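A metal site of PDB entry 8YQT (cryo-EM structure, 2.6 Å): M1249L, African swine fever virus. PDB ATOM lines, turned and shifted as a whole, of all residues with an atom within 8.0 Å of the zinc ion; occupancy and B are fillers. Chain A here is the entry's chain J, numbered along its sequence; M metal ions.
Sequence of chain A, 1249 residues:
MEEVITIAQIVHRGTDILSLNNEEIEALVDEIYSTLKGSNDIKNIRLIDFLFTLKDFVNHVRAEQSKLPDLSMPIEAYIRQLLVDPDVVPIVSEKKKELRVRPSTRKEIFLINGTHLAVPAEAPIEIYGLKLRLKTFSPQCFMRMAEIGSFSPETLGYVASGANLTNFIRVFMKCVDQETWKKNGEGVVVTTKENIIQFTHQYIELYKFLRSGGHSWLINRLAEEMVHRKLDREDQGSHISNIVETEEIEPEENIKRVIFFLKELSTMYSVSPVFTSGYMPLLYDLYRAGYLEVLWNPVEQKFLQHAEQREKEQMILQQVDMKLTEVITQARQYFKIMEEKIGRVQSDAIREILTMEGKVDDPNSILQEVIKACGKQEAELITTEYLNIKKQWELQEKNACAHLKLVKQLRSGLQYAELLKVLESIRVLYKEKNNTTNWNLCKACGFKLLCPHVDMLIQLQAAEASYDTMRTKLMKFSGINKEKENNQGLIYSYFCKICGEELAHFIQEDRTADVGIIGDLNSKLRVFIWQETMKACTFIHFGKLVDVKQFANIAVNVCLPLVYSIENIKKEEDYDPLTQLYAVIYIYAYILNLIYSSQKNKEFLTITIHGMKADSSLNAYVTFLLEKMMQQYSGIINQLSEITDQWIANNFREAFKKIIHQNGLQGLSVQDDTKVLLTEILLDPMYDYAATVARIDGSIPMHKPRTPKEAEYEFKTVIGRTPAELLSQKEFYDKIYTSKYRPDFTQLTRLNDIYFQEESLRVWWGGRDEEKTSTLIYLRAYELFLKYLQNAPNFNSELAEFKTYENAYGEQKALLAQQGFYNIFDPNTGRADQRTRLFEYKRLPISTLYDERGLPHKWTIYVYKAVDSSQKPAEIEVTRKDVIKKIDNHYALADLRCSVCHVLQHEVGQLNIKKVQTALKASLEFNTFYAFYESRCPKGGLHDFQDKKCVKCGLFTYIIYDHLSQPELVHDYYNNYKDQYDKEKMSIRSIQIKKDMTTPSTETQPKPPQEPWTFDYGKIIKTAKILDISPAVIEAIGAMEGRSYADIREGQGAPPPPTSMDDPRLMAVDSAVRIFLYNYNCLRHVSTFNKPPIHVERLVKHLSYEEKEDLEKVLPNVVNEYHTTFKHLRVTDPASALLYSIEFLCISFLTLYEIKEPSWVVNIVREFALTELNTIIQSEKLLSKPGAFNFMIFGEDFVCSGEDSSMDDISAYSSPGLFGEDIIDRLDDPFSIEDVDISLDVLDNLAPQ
The zinc ion is bound by a ring nitrogen (ND1) of His 943 (2.3 Å), the side-chain sulfur (SG) of Cys 950 (2.3 Å) and the side-chain sulfur (SG) of Cys 937 (2.3 Å).
The zinc ion has three donor atoms within binding distance.
Merely in contact with the zinc ion: Cys 953 (3.2 Å).
Within 4 Å of the zinc ion: Cys 937, His 943, Cys 950 and Cys 953.
O of Leu 955 lies within hydrogen-bond range of N of Cys 950 (2.7 Å).
The side-chain hydroxyl (OH) of Tyr 977 lies within hydrogen-bond range of the side-chain sulfur (SG) of Cys 953, at 3.7 Å.
A ring nitrogen (NE2) of His 943 lies within hydrogen-bond range of the backbone carbonyl oxygen (O) of Arg 936, 2.6 Å away.
N of Lys 939 lies close to SG of Cys 937, 3.7 Å away.
N of Asp 944 sits close to SG of Cys 950.
SG of Cys 950 sits close to N of Lys 952 (3.5 Å).
N of Cys 953 sits close to SG of Cys 950 (3.6 Å).
O of Ser 935 is in hydrogen-bond range of N of His 943, at 3.3 Å.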
ATOM      1  N   TYR A 933      11.472   1.298 -33.717  1.00  0.00           N
ATOM      2  CA  TYR A 933      11.802   0.138 -32.881  1.00  0.00           C
ATOM      3  C   TYR A 933      13.265   0.136 -32.462  1.00  0.00           C
ATOM      4  O   TYR A 933      13.961  -0.857 -32.595  1.00  0.00           O
ATOM      5  CB  TYR A 933      11.455  -1.144 -33.625  1.00  0.00           C
ATOM      6  CG  TYR A 933       9.983  -1.493 -33.603  1.00  0.00           C
ATOM      7  CD1 TYR A 933       9.189  -1.174 -32.513  1.00  0.00           C
ATOM      8  CD2 TYR A 933       9.393  -2.158 -34.672  1.00  0.00           C
ATOM      9  CE1 TYR A 933       7.850  -1.491 -32.493  1.00  0.00           C
ATOM     10  CE2 TYR A 933       8.058  -2.483 -34.655  1.00  0.00           C
ATOM     11  CZ  TYR A 933       7.291  -2.144 -33.560  1.00  0.00           C
ATOM     12  OH  TYR A 933       5.951  -2.461 -33.539  1.00  0.00           O
ATOM     13  N   GLU A 934      13.739   1.258 -31.919  1.00  0.00           N
ATOM     14  CA  GLU A 934      15.071   1.300 -31.331  1.00  0.00           C
ATOM     15  C   GLU A 934      15.058   1.263 -29.821  1.00  0.00           C
ATOM     16  O   GLU A 934      15.902   0.598 -29.212  1.00  0.00           O
ATOM     17  CB  GLU A 934      15.838   2.540 -31.820  1.00  0.00           C
ATOM     18  CG  GLU A 934      15.268   3.864 -31.374  1.00  0.00           C
ATOM     19  CD  GLU A 934      16.224   5.010 -31.644  1.00  0.00           C
ATOM     20  OE1 GLU A 934      17.293   4.766 -32.243  1.00  0.00           O
ATOM     21  OE2 GLU A 934      15.917   6.158 -31.270  1.00  0.00           O
ATOM     22  N   SER A 935      14.109   1.953 -29.187  1.00  0.00           N
ATOM     23  CA  SER A 935      13.770   1.751 -27.789  1.00  0.00           C
ATOM     24  C   SER A 935      12.451   1.040 -27.611  1.00  0.00           C
ATOM     25  O   SER A 935      12.305   0.250 -26.679  1.00  0.00           O
ATOM     26  CB  SER A 935      13.721   3.095 -27.051  1.00  0.00           C
ATOM     27  OG  SER A 935      14.997   3.722 -27.033  1.00  0.00           O
ATOM     28  N   ARG A 936      11.484   1.306 -28.486  1.00  0.00           N
ATOM     29  CA  ARG A 936      10.251   0.543 -28.527  1.00  0.00           C
ATOM     30  C   ARG A 936      10.554  -0.934 -28.704  1.00  0.00           C
ATOM     31  O   ARG A 936      11.331  -1.312 -29.578  1.00  0.00           O
ATOM     32  CB  ARG A 936       9.362   1.022 -29.688  1.00  0.00           C
ATOM     33  CG  ARG A 936       8.299   2.039 -29.349  1.00  0.00           C
ATOM     34  CD  ARG A 936       8.916   3.338 -28.959  1.00  0.00           C
ATOM     35  NE  ARG A 936       8.028   4.473 -29.176  1.00  0.00           N
ATOM     36  CZ  ARG A 936       8.221   5.396 -30.100  1.00  0.00           C
ATOM     37  NH1 ARG A 936       9.246   5.330 -30.944  1.00  0.00           N
ATOM     38  NH2 ARG A 936       7.380   6.421 -30.189  1.00  0.00           N
ATOM     39  N   CYS A 937       9.958  -1.747 -27.893  1.00  0.00           N
ATOM     40  CA  CYS A 937      10.076  -3.159 -28.197  1.00  0.00           C
ATOM     41  C   CYS A 937       8.791  -3.663 -28.838  1.00  0.00           C
ATOM     42  O   CYS A 937       7.705  -3.396 -28.303  1.00  0.00           O
ATOM     43  CB  CYS A 937      10.385  -3.967 -26.945  1.00  0.00           C
ATOM     44  SG  CYS A 937      10.929  -5.656 -27.262  1.00  0.00           S
ATOM     45  N   PRO A 938       8.869  -4.348 -29.980  1.00  0.00           N
ATOM     46  CA  PRO A 938       7.655  -4.933 -30.562  1.00  0.00           C
ATOM     47  C   PRO A 938       6.928  -5.879 -29.633  1.00  0.00           C
ATOM     48  O   PRO A 938       5.701  -6.044 -29.762  1.00  0.00           O
ATOM     49  CB  PRO A 938       8.170  -5.659 -31.810  1.00  0.00           C
ATOM     50  CG  PRO A 938       9.404  -4.921 -32.169  1.00  0.00           C
ATOM     51  CD  PRO A 938      10.017  -4.437 -30.893  1.00  0.00           C
ATOM     52  N   LYS A 939       7.636  -6.525 -28.704  1.00  0.00           N
ATOM     53  CA  LYS A 939       7.005  -7.367 -27.685  1.00  0.00           C
ATOM     54  C   LYS A 939       6.597  -6.583 -26.442  1.00  0.00           C
ATOM     55  O   LYS A 939       6.439  -7.172 -25.368  1.00  0.00           O
ATOM     56  CB  LYS A 939       7.943  -8.518 -27.314  1.00  0.00           C
ATOM     57  CG  LYS A 939       8.273  -9.443 -28.475  1.00  0.00           C
ATOM     58  CD  LYS A 939       7.025 -10.087 -29.037  1.00  0.00           C
ATOM     59  CE  LYS A 939       7.367 -11.025 -30.185  1.00  0.00           C
ATOM     60  NZ  LYS A 939       6.148 -11.620 -30.801  1.00  0.00           N
ATOM     61  N   GLY A 940       6.442  -5.269 -26.567  1.00  0.00           N
ATOM     62  CA  GLY A 940       5.966  -4.448 -25.464  1.00  0.00           C
ATOM     63  C   GLY A 940       7.094  -3.902 -24.622  1.00  0.00           C
ATOM     64  O   GLY A 940       8.160  -4.493 -24.479  1.00  0.00           O
ATOM     65  N   GLY A 941       6.847  -2.726 -24.052  1.00  0.00           N
ATOM     66  CA  GLY A 941       7.858  -2.112 -23.208  1.00  0.00           C
ATOM     67  C   GLY A 941       9.057  -1.656 -24.006  1.00  0.00           C
ATOM     68  O   GLY A 941       8.978  -1.305 -25.184  1.00  0.00           O
ATOM     69  N   LEU A 942      10.209  -1.652 -23.343  1.00  0.00           N
ATOM     70  CA  LEU A 942      11.484  -1.288 -23.952  1.00  0.00           C
ATOM     71  C   LEU A 942      12.351  -2.527 -24.116  1.00  0.00           C
ATOM     72  O   LEU A 942      12.096  -3.576 -23.506  1.00  0.00           O
ATOM     73  CB  LEU A 942      12.194  -0.221 -23.108  1.00  0.00           C
ATOM     74  CG  LEU A 942      11.331   0.992 -22.762  1.00  0.00           C
ATOM     75  CD1 LEU A 942      12.104   1.972 -21.902  1.00  0.00           C
ATOM     76  CD2 LEU A 942      10.835   1.667 -24.019  1.00  0.00           C
ATOM     77  N   HIS A 943      13.379  -2.391 -24.935  1.00  0.00           N
ATOM     78  CA  HIS A 943      14.227  -3.531 -25.276  1.00  0.00           C
ATOM     79  C   HIS A 943      15.013  -4.007 -24.060  1.00  0.00           C
ATOM     80  O   HIS A 943      15.359  -3.234 -23.160  1.00  0.00           O
ATOM     81  CB  HIS A 943      15.183  -3.175 -26.405  1.00  0.00           C
ATOM     82  CG  HIS A 943      14.519  -3.051 -27.741  1.00  0.00           C
ATOM     83  ND1 HIS A 943      13.962  -4.117 -28.402  1.00  0.00           N
ATOM     84  CD2 HIS A 943      14.334  -1.968 -28.538  1.00  0.00           C
ATOM     85  CE1 HIS A 943      13.461  -3.706 -29.554  1.00  0.00           C
ATOM     86  NE2 HIS A 943      13.672  -2.414 -29.659  1.00  0.00           N
ATOM     87  N   ASP A 944      15.297  -5.311 -24.044  1.00  0.00           N
ATOM     88  CA  ASP A 944      16.056  -5.958 -22.967  1.00  0.00           C
ATOM     89  C   ASP A 944      17.316  -6.498 -23.621  1.00  0.00           C
ATOM     90  O   ASP A 944      17.329  -7.621 -24.134  1.00  0.00           O
ATOM     91  CB  ASP A 944      15.207  -7.054 -22.279  1.00  0.00           C
ATOM     92  CG  ASP A 944      15.990  -7.879 -21.253  1.00  0.00           C
ATOM     93  OD1 ASP A 944      15.343  -8.349 -20.288  1.00  0.00           O
ATOM     94  OD2 ASP A 944      17.205  -8.080 -21.385  1.00  0.00           O
ATOM     95  N   PHE A 945      18.388  -5.709 -23.605  1.00  0.00           N
ATOM     96  CA  PHE A 945      19.666  -6.103 -24.201  1.00  0.00           C
ATOM     97  C   PHE A 945      20.507  -6.808 -23.154  1.00  0.00           C
ATOM     98  O   PHE A 945      21.199  -6.147 -22.364  1.00  0.00           O
ATOM     99  CB  PHE A 945      20.404  -4.888 -24.763  1.00  0.00           C
ATOM    100  CG  PHE A 945      19.702  -4.203 -25.897  1.00  0.00           C
ATOM    101  CD1 PHE A 945      19.579  -4.814 -27.124  1.00  0.00           C
ATOM    102  CD2 PHE A 945      19.191  -2.927 -25.726  1.00  0.00           C
ATOM    103  CE1 PHE A 945      18.925  -4.174 -28.168  1.00  0.00           C
ATOM    104  CE2 PHE A 945      18.550  -2.286 -26.763  1.00  0.00           C
ATOM    105  CZ  PHE A 945      18.425  -2.912 -27.983  1.00  0.00           C
ATOM    106  N   LYS A 949      22.011  -8.575 -28.828  1.00  0.00           N
ATOM    107  CA  LYS A 949      20.669  -8.966 -29.232  1.00  0.00           C
ATOM    108  C   LYS A 949      19.692  -8.791 -28.073  1.00  0.00           C
ATOM    109  O   LYS A 949      19.984  -9.216 -26.950  1.00  0.00           O
ATOM    110  CB  LYS A 949      20.665 -10.413 -29.720  1.00  0.00           C
ATOM    111  CG  LYS A 949      19.320 -10.929 -30.214  1.00  0.00           C
ATOM    112  CD  LYS A 949      19.460 -12.331 -30.772  1.00  0.00           C
ATOM    113  CE  LYS A 949      18.132 -12.877 -31.261  1.00  0.00           C
ATOM    114  NZ  LYS A 949      18.271 -14.214 -31.911  1.00  0.00           N
ATOM    115  N   CYS A 950      18.547  -8.182 -28.347  1.00  0.00           N
ATOM    116  CA  CYS A 950      17.483  -8.058 -27.359  1.00  0.00           C
ATOM    117  C   CYS A 950      16.945  -9.440 -26.996  1.00  0.00           C
ATOM    118  O   CYS A 950      17.021 -10.393 -27.767  1.00  0.00           O
ATOM    119  CB  CYS A 950      16.356  -7.172 -27.885  1.00  0.00           C
ATOM    120  SG  CYS A 950      14.916  -7.021 -26.808  1.00  0.00           S
ATOM    121  N   VAL A 951      16.404  -9.548 -25.778  1.00  0.00           N
ATOM    122  CA  VAL A 951      15.885 -10.815 -25.289  1.00  0.00           C
ATOM    123  C   VAL A 951      14.438 -11.034 -25.700  1.00  0.00           C
ATOM    124  O   VAL A 951      14.071 -12.127 -26.134  1.00  0.00           O
ATOM    125  CB  VAL A 951      16.061 -10.890 -23.757  1.00  0.00           C
ATOM    126  CG1 VAL A 951      15.246 -12.045 -23.190  1.00  0.00           C
ATOM    127  CG2 VAL A 951      17.518 -11.036 -23.389  1.00  0.00           C
ATOM    128  N   LYS A 952      13.601 -10.001 -25.575  1.00  0.00           N
ATOM    129  CA  LYS A 952      12.193 -10.141 -25.945  1.00  0.00           C
ATOM    130  C   LYS A 952      12.011 -10.282 -27.449  1.00  0.00           C
ATOM    131  O   LYS A 952      11.102 -10.979 -27.899  1.00  0.00           O
ATOM    132  CB  LYS A 952      11.394  -8.954 -25.409  1.00  0.00           C
ATOM    133  CG  LYS A 952      11.474  -8.798 -23.903  1.00  0.00           C
ATOM    134  CD  LYS A 952      10.384  -7.879 -23.380  1.00  0.00           C
ATOM    135  CE  LYS A 952      10.640  -6.439 -23.764  1.00  0.00           C
ATOM    136  NZ  LYS A 952      11.846  -5.884 -23.098  1.00  0.00           N
ATOM    137  N   CYS A 953      12.858  -9.616 -28.228  1.00  0.00           N
ATOM    138  CA  CYS A 953      12.828  -9.645 -29.684  1.00  0.00           C
ATOM    139  C   CYS A 953      14.144 -10.225 -30.204  1.00  0.00           C
ATOM    140  O   CYS A 953      14.959 -10.744 -29.452  1.00  0.00           O
ATOM    141  CB  CYS A 953      12.560  -8.253 -30.255  1.00  0.00           C
ATOM    142  SG  CYS A 953      10.836  -7.759 -30.218  1.00  0.00           S
ATOM    143  N   GLY A 954      14.328 -10.150 -31.518  1.00  0.00           N
ATOM    144  CA  GLY A 954      15.573 -10.553 -32.125  1.00  0.00           C
ATOM    145  C   GLY A 954      16.365  -9.384 -32.667  1.00  0.00           C
ATOM    146  O   GLY A 954      17.064  -9.510 -33.672  1.00  0.00           O
ATOM    147  N   LEU A 955      16.266  -8.224 -32.006  1.00  0.00           N
ATOM    148  CA  LEU A 955      16.915  -7.017 -32.477  1.00  0.00           C
ATOM    149  C   LEU A 955      18.378  -7.007 -32.033  1.00  0.00           C
ATOM    150  O   LEU A 955      18.666  -7.089 -30.842  1.00  0.00           O
ATOM    151  CB  LEU A 955      16.203  -5.769 -31.971  1.00  0.00           C
ATOM    152  CG  LEU A 955      16.872  -4.450 -32.362  1.00  0.00           C
ATOM    153  CD1 LEU A 955      16.851  -4.262 -33.871  1.00  0.00           C
ATOM    154  CD2 LEU A 955      16.229  -3.276 -31.659  1.00  0.00           C
ATOM    155  N   TYR A 973      14.383  -9.135 -39.366  1.00  0.00           N
ATOM    156  CA  TYR A 973      13.696  -8.402 -38.313  1.00  0.00           C
ATOM    157  C   TYR A 973      12.571  -7.557 -38.874  1.00  0.00           C
ATOM    158  O   TYR A 973      11.438  -7.582 -38.360  1.00  0.00           O
ATOM    159  CB  TYR A 973      14.705  -7.522 -37.559  1.00  0.00           C
ATOM    160  CG  TYR A 973      14.139  -6.826 -36.343  1.00  0.00           C
ATOM    161  CD1 TYR A 973      14.043  -7.481 -35.123  1.00  0.00           C
ATOM    162  CD2 TYR A 973      13.704  -5.511 -36.417  1.00  0.00           C
ATOM    163  CE1 TYR A 973      13.528  -6.844 -34.014  1.00  0.00           C
ATOM    164  CE2 TYR A 973      13.198  -4.869 -35.309  1.00  0.00           C
ATOM    165  CZ  TYR A 973      13.114  -5.534 -34.109  1.00  0.00           C
ATOM    166  OH  TYR A 973      12.595  -4.895 -33.008  1.00  0.00           O
ATOM    167  N   TYR A 977       8.168  -7.995 -37.725  1.00  0.00           N
ATOM    168  CA  TYR A 977       7.331  -7.055 -36.997  1.00  0.00           C
ATOM    169  C   TYR A 977       6.860  -5.930 -37.909  1.00  0.00           C
ATOM    170  O   TYR A 977       6.911  -4.749 -37.564  1.00  0.00           O
ATOM    171  CB  TYR A 977       8.089  -6.510 -35.798  1.00  0.00           C
ATOM    172  CG  TYR A 977       8.670  -7.596 -34.921  1.00  0.00           C
ATOM    173  CD1 TYR A 977       7.873  -8.344 -34.075  1.00  0.00           C
ATOM    174  CD2 TYR A 977      10.037  -7.878 -34.949  1.00  0.00           C
ATOM    175  CE1 TYR A 977       8.397  -9.344 -33.283  1.00  0.00           C
ATOM    176  CE2 TYR A 977      10.570  -8.873 -34.160  1.00  0.00           C
ATOM    177  CZ  TYR A 977       9.746  -9.601 -33.330  1.00  0.00           C
ATOM    178  OH  TYR A 977      10.291 -10.594 -32.534  1.00  0.00           O
HETATM  179 ZN    ZN M   1      13.079  -6.177 -27.902  1.00  0.00          ZN
